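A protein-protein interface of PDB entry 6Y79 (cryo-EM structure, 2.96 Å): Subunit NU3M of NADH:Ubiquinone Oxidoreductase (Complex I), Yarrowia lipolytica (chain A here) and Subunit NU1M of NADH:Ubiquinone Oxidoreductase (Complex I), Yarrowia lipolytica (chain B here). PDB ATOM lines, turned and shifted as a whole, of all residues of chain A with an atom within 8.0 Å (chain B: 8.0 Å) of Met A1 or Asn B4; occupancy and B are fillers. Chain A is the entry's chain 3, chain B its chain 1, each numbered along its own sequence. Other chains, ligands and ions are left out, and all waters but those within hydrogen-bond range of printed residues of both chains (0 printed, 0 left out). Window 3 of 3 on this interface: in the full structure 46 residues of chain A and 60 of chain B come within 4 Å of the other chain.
Printed residues of chain B that touch a printed residue of chain A: Asn B4, Ile B5, Ile B8 and Leu B99.
Hydrophobic or aromatic side chains of chain B within 4 Å of the printed part of chain A: Ile B5, Ile B8 and Leu B99.
Hydrophobic or aromatic side chains of chain A that line the printed part of chain B: Phe A4, Ile A6 and Phe A7.
Among the printed residues, 11 pairs touch across the chains.
Among the printed residues, no Asp or Glu carboxylate lies within 4 Å of a Lys or Arg side-chain nitrogen of the other chain.
The side-chain amide oxygen (OD1) of Asn B4 lies close to the backbone carbonyl oxygen (O) of Met B1 (2.8 Å).
OD1 of Asn A2 sits close to N of Phe A4, 3.4 Å away.
The side-chain amide oxygen (OD1) of Asn A2 lies close to the backbone NH (N) of Ile A5.
The side-chain amide nitrogen of Asn B4 lies within hydrogen-bond range of the backbone carbonyl oxygen of Met A1, at 2.9 Å.
O of Leu B99 sits at hydrogen-bond distance from N of Phe A4, at 3.1 Å.
The backbone carbonyl oxygen of Leu B99 lies close to the backbone carbonyl oxygen of Thr A3 (3.1 Å).
Asn A2 touches Asn B4 (O to ND2, 3.7 Å).
OG1 of Thr A3 touches O of Asn B4 (3.8 Å).
O of Thr A3 touches CD1 of Ile B8, 3.4 Å away.
Asn B4 touches Ile A6 (ND2 to CD1, 3.7 Å).
Ile B5 touches Ile A6.
Ile A6 touches Ile B8.
N of Phe A7 touches CD1 of Ile B8, at 3.3 Å.
Phe A7 touches Leu B99.
Of chain B, only Asn B4 comes within 4 Å of Met A1.
Printed residues of chain B within 4 Å of Thr A3: Asn B4, Ile B8 and Leu B99.
Of the printed residues of chain B, Ile A6 touches Asn B4, Ile B5 and Ile B8.
Ile B2 touches none of the printed residues of chain A.
Asn B4 touches just these residues of chain A: Met A1, Asn A2, Thr A3 and Ile A6.
Leu B9 touches none of the printed residues of chain A.
The nearest residue of chain B that does not touch Met A1 is Met B1 (4.6 Å).
The nearest residue of chain A that does not touch Asn B4 is Phe A4 (6.4 Å).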
ATOM      1  N   MET A   1     -28.225 -11.666  10.917  1.00  0.00           N
ATOM      2  CA  MET A   1     -29.368 -11.482  11.808  1.00  0.00           C
ATOM      3  C   MET A   1     -29.998 -12.800  12.222  1.00  0.00           C
ATOM      4  O   MET A   1     -31.038 -12.811  12.869  1.00  0.00           O
ATOM      5  CB  MET A   1     -30.427 -10.580  11.154  1.00  0.00           C
ATOM      6  CG  MET A   1     -30.985 -11.022   9.782  1.00  0.00           C
ATOM      7  SD  MET A   1     -32.318 -12.233   9.764  1.00  0.00           S
ATOM      8  CE  MET A   1     -33.636 -11.313  10.558  1.00  0.00           C
ATOM      9  N   ASN A   2     -29.376 -13.911  11.858  1.00  0.00           N
ATOM     10  CA  ASN A   2     -29.847 -15.193  12.346  1.00  0.00           C
ATOM     11  C   ASN A   2     -29.254 -15.453  13.720  1.00  0.00           C
ATOM     12  O   ASN A   2     -28.423 -14.699  14.223  1.00  0.00           O
ATOM     13  CB  ASN A   2     -29.525 -16.339  11.368  1.00  0.00           C
ATOM     14  CG  ASN A   2     -28.046 -16.441  11.001  1.00  0.00           C
ATOM     15  OD1 ASN A   2     -27.188 -15.760  11.555  1.00  0.00           O
ATOM     16  ND2 ASN A   2     -27.749 -17.320  10.052  1.00  0.00           N
ATOM     17  N   THR A   3     -29.677 -16.550  14.323  1.00  0.00           N
ATOM     18  CA  THR A   3     -29.133 -16.958  15.604  1.00  0.00           C
ATOM     19  C   THR A   3     -27.824 -17.739  15.458  1.00  0.00           C
ATOM     20  O   THR A   3     -27.322 -18.276  16.446  1.00  0.00           O
ATOM     21  CB  THR A   3     -30.198 -17.741  16.377  1.00  0.00           C
ATOM     22  OG1 THR A   3     -29.632 -18.310  17.566  1.00  0.00           O
ATOM     23  CG2 THR A   3     -30.871 -18.801  15.494  1.00  0.00           C
ATOM     24  N   PHE A   4     -27.257 -17.788  14.246  1.00  0.00           N
ATOM     25  CA  PHE A   4     -25.995 -18.473  13.973  1.00  0.00           C
ATOM     26  C   PHE A   4     -24.785 -17.602  14.278  1.00  0.00           C
ATOM     27  O   PHE A   4     -23.761 -18.119  14.731  1.00  0.00           O
ATOM     28  CB  PHE A   4     -25.964 -18.908  12.502  1.00  0.00           C
ATOM     29  CG  PHE A   4     -24.730 -19.670  12.100  1.00  0.00           C
ATOM     30  CD1 PHE A   4     -24.607 -21.004  12.406  1.00  0.00           C
ATOM     31  CD2 PHE A   4     -23.709 -19.058  11.389  1.00  0.00           C
ATOM     32  CE1 PHE A   4     -23.480 -21.721  12.043  1.00  0.00           C
ATOM     33  CE2 PHE A   4     -22.576 -19.771  11.018  1.00  0.00           C
ATOM     34  CZ  PHE A   4     -22.466 -21.103  11.346  1.00  0.00           C
ATOM     35  N   ILE A   5     -24.892 -16.290  14.057  1.00  0.00           N
ATOM     36  CA  ILE A   5     -23.740 -15.393  14.073  1.00  0.00           C
ATOM     37  C   ILE A   5     -23.522 -14.741  15.437  1.00  0.00           C
ATOM     38  O   ILE A   5     -22.365 -14.457  15.796  1.00  0.00           O
ATOM     39  CB  ILE A   5     -23.904 -14.343  12.952  1.00  0.00           C
ATOM     40  CG1 ILE A   5     -23.990 -15.060  11.611  1.00  0.00           C
ATOM     41  CG2 ILE A   5     -22.742 -13.361  12.859  1.00  0.00           C
ATOM     42  CD1 ILE A   5     -24.356 -14.163  10.471  1.00  0.00           C
ATOM     43  N   ILE A   6     -24.588 -14.544  16.225  1.00  0.00           N
ATOM     44  CA  ILE A   6     -24.467 -14.116  17.619  1.00  0.00           C
ATOM     45  C   ILE A   6     -23.619 -15.105  18.407  1.00  0.00           C
ATOM     46  O   ILE A   6     -22.857 -14.722  19.298  1.00  0.00           O
ATOM     47  CB  ILE A   6     -25.870 -13.963  18.236  1.00  0.00           C
ATOM     48  CG1 ILE A   6     -26.797 -13.240  17.258  1.00  0.00           C
ATOM     49  CG2 ILE A   6     -25.795 -13.244  19.586  1.00  0.00           C
ATOM     50  CD1 ILE A   6     -28.258 -13.415  17.563  1.00  0.00           C
ATOM     51  N   PHE A   7     -23.694 -16.384  18.038  1.00  0.00           N
ATOM     52  CA  PHE A   7     -22.856 -17.424  18.623  1.00  0.00           C
ATOM     53  C   PHE A   7     -21.392 -17.223  18.271  1.00  0.00           C
ATOM     54  O   PHE A   7     -20.521 -17.218  19.158  1.00  0.00           O
ATOM     55  CB  PHE A   7     -23.341 -18.764  18.107  1.00  0.00           C
ATOM     56  CG  PHE A   7     -22.900 -19.910  18.914  1.00  0.00           C
ATOM     57  CD1 PHE A   7     -23.549 -20.233  20.083  1.00  0.00           C
ATOM     58  CD2 PHE A   7     -21.826 -20.662  18.515  1.00  0.00           C
ATOM     59  CE1 PHE A   7     -23.159 -21.317  20.820  1.00  0.00           C
ATOM     60  CE2 PHE A   7     -21.441 -21.738  19.233  1.00  0.00           C
ATOM     61  CZ  PHE A   7     -22.099 -22.066  20.399  1.00  0.00           C
ATOM     62  N   MET B   1     -35.962 -10.039  16.615  1.00  0.00           N
ATOM     63  CA  MET B   1     -34.579  -9.865  17.047  1.00  0.00           C
ATOM     64  C   MET B   1     -34.497 -10.008  18.566  1.00  0.00           C
ATOM     65  O   MET B   1     -33.443 -10.306  19.131  1.00  0.00           O
ATOM     66  CB  MET B   1     -34.036  -8.510  16.576  1.00  0.00           C
ATOM     67  CG  MET B   1     -32.549  -8.282  16.842  1.00  0.00           C
ATOM     68  SD  MET B   1     -31.456  -9.155  15.706  1.00  0.00           S
ATOM     69  CE  MET B   1     -29.859  -8.701  16.379  1.00  0.00           C
ATOM     70  N   ILE B   2     -35.625  -9.805  19.240  1.00  0.00           N
ATOM     71  CA  ILE B   2     -35.697 -10.227  20.630  1.00  0.00           C
ATOM     72  C   ILE B   2     -35.692 -11.748  20.687  1.00  0.00           C
ATOM     73  O   ILE B   2     -35.043 -12.343  21.565  1.00  0.00           O
ATOM     74  CB  ILE B   2     -36.942  -9.610  21.297  1.00  0.00           C
ATOM     75  CG1 ILE B   2     -36.907  -8.084  21.153  1.00  0.00           C
ATOM     76  CG2 ILE B   2     -37.030  -9.990  22.761  1.00  0.00           C
ATOM     77  CD1 ILE B   2     -35.712  -7.429  21.805  1.00  0.00           C
ATOM     78  N   ILE B   3     -36.308 -12.375  19.680  1.00  0.00           N
ATOM     79  CA  ILE B   3     -36.554 -13.810  19.655  1.00  0.00           C
ATOM     80  C   ILE B   3     -35.250 -14.600  19.554  1.00  0.00           C
ATOM     81  O   ILE B   3     -35.007 -15.528  20.329  1.00  0.00           O
ATOM     82  CB  ILE B   3     -37.500 -14.110  18.476  1.00  0.00           C
ATOM     83  CG1 ILE B   3     -38.643 -13.063  18.387  1.00  0.00           C
ATOM     84  CG2 ILE B   3     -38.035 -15.515  18.564  1.00  0.00           C
ATOM     85  CD1 ILE B   3     -39.613 -13.028  19.559  1.00  0.00           C
ATOM     86  N   ASN B   4     -34.373 -14.238  18.627  1.00  0.00           N
ATOM     87  CA  ASN B   4     -33.181 -15.052  18.426  1.00  0.00           C
ATOM     88  C   ASN B   4     -32.122 -14.827  19.497  1.00  0.00           C
ATOM     89  O   ASN B   4     -31.397 -15.766  19.836  1.00  0.00           O
ATOM     90  CB  ASN B   4     -32.621 -14.816  17.023  1.00  0.00           C
ATOM     91  CG  ASN B   4     -32.209 -13.389  16.801  1.00  0.00           C
ATOM     92  OD1 ASN B   4     -32.588 -12.498  17.557  1.00  0.00           O
ATOM     93  ND2 ASN B   4     -31.452 -13.150  15.746  1.00  0.00           N
ATOM     94  N   ILE B   5     -32.036 -13.625  20.067  1.00  0.00           N
ATOM     95  CA  ILE B   5     -31.032 -13.437  21.099  1.00  0.00           C
ATOM     96  C   ILE B   5     -31.510 -14.052  22.416  1.00  0.00           C
ATOM     97  O   ILE B   5     -30.691 -14.601  23.178  1.00  0.00           O
ATOM     98  CB  ILE B   5     -30.638 -11.955  21.236  1.00  0.00           C
ATOM     99  CG1 ILE B   5     -30.325 -11.391  19.856  1.00  0.00           C
ATOM    100  CG2 ILE B   5     -29.413 -11.818  22.158  1.00  0.00           C
ATOM    101  CD1 ILE B   5     -29.369 -10.197  19.798  1.00  0.00           C
ATOM    102  N   VAL B   6     -32.832 -14.057  22.675  1.00  0.00           N
ATOM    103  CA  VAL B   6     -33.287 -14.793  23.856  1.00  0.00           C
ATOM    104  C   VAL B   6     -33.076 -16.290  23.642  1.00  0.00           C
ATOM    105  O   VAL B   6     -32.601 -16.970  24.553  1.00  0.00           O
ATOM    106  CB  VAL B   6     -34.742 -14.437  24.282  1.00  0.00           C
ATOM    107  CG1 VAL B   6     -35.820 -14.943  23.355  1.00  0.00           C
ATOM    108  CG2 VAL B   6     -35.024 -14.984  25.665  1.00  0.00           C
ATOM    109  N   GLU B   7     -33.270 -16.791  22.410  1.00  0.00           N
ATOM    110  CA  GLU B   7     -33.015 -18.204  22.119  1.00  0.00           C
ATOM    111  C   GLU B   7     -31.541 -18.572  22.281  1.00  0.00           C
ATOM    112  O   GLU B   7     -31.215 -19.629  22.840  1.00  0.00           O
ATOM    113  CB  GLU B   7     -33.488 -18.534  20.705  1.00  0.00           C
ATOM    114  CG  GLU B   7     -33.155 -19.937  20.257  1.00  0.00           C
ATOM    115  CD  GLU B   7     -33.577 -20.197  18.835  1.00  0.00           C
ATOM    116  OE1 GLU B   7     -33.361 -21.326  18.344  1.00  0.00           O
ATOM    117  OE2 GLU B   7     -34.124 -19.267  18.206  1.00  0.00           O
ATOM    118  N   ILE B   8     -30.634 -17.701  21.843  1.00  0.00           N
ATOM    119  CA  ILE B   8     -29.232 -18.075  21.889  1.00  0.00           C
ATOM    120  C   ILE B   8     -28.668 -17.963  23.304  1.00  0.00           C
ATOM    121  O   ILE B   8     -27.820 -18.768  23.692  1.00  0.00           O
ATOM    122  CB  ILE B   8     -28.419 -17.267  20.866  1.00  0.00           C
ATOM    123  CG1 ILE B   8     -27.037 -17.849  20.754  1.00  0.00           C
ATOM    124  CG2 ILE B   8     -28.265 -15.817  21.236  1.00  0.00           C
ATOM    125  CD1 ILE B   8     -26.388 -17.391  19.604  1.00  0.00           C
ATOM    126  N   LEU B   9     -29.138 -17.025  24.132  1.00  0.00           N
ATOM    127  CA  LEU B   9     -28.641 -17.005  25.503  1.00  0.00           C
ATOM    128  C   LEU B   9     -29.312 -18.080  26.355  1.00  0.00           C
ATOM    129  O   LEU B   9     -28.711 -18.530  27.339  1.00  0.00           O
ATOM    130  CB  LEU B   9     -28.787 -15.615  26.123  1.00  0.00           C
ATOM    131  CG  LEU B   9     -27.531 -14.738  25.910  1.00  0.00           C
ATOM    132  CD1 LEU B   9     -26.231 -15.463  26.319  1.00  0.00           C
ATOM    133  CD2 LEU B   9     -27.403 -14.149  24.509  1.00  0.00           C
ATOM    134  N   ILE B  10     -30.509 -18.564  25.950  1.00  0.00           N
ATOM    135  CA  ILE B  10     -31.038 -19.793  26.550  1.00  0.00           C
ATOM    136  C   ILE B  10     -30.167 -21.005  26.195  1.00  0.00           C
ATOM    137  O   ILE B  10     -29.836 -21.817  27.073  1.00  0.00           O
ATOM    138  CB  ILE B  10     -32.504 -20.031  26.143  1.00  0.00           C
ATOM    139  CG1 ILE B  10     -33.482 -19.016  26.750  1.00  0.00           C
ATOM    140  CG2 ILE B  10     -32.995 -21.410  26.553  1.00  0.00           C
ATOM    141  CD1 ILE B  10     -33.217 -18.608  28.177  1.00  0.00           C
ATOM    142  N   PHE B  11     -29.750 -21.135  24.933  1.00  0.00           N
ATOM    143  CA  PHE B  11     -28.890 -22.260  24.564  1.00  0.00           C
ATOM    144  C   PHE B  11     -27.524 -22.164  25.231  1.00  0.00           C
ATOM    145  O   PHE B  11     -26.977 -23.183  25.674  1.00  0.00           O
ATOM    146  CB  PHE B  11     -28.722 -22.357  23.045  1.00  0.00           C
ATOM    147  CG  PHE B  11     -27.987 -23.592  22.593  1.00  0.00           C
ATOM    148  CD1 PHE B  11     -28.655 -24.792  22.446  1.00  0.00           C
ATOM    149  CD2 PHE B  11     -26.628 -23.558  22.339  1.00  0.00           C
ATOM    150  CE1 PHE B  11     -27.989 -25.923  22.031  1.00  0.00           C
ATOM    151  CE2 PHE B  11     -25.959 -24.683  21.916  1.00  0.00           C
ATOM    152  CZ  PHE B  11     -26.643 -25.867  21.767  1.00  0.00           C
ATOM    153  N   LEU B  99     -29.132 -23.690  16.404  1.00  0.00           N
ATOM    154  CA  LEU B  99     -28.806 -22.279  16.339  1.00  0.00           C
ATOM    155  C   LEU B  99     -28.474 -21.826  14.935  1.00  0.00           C
ATOM    156  O   LEU B  99     -28.358 -20.640  14.697  1.00  0.00           O
ATOM    157  CB  LEU B  99     -27.620 -21.965  17.221  1.00  0.00           C
ATOM    158  CG  LEU B  99     -27.747 -22.366  18.661  1.00  0.00           C
ATOM    159  CD1 LEU B  99     -26.471 -21.954  19.252  1.00  0.00           C
ATOM    160  CD2 LEU B  99     -28.903 -21.654  19.324  1.00  0.00           C
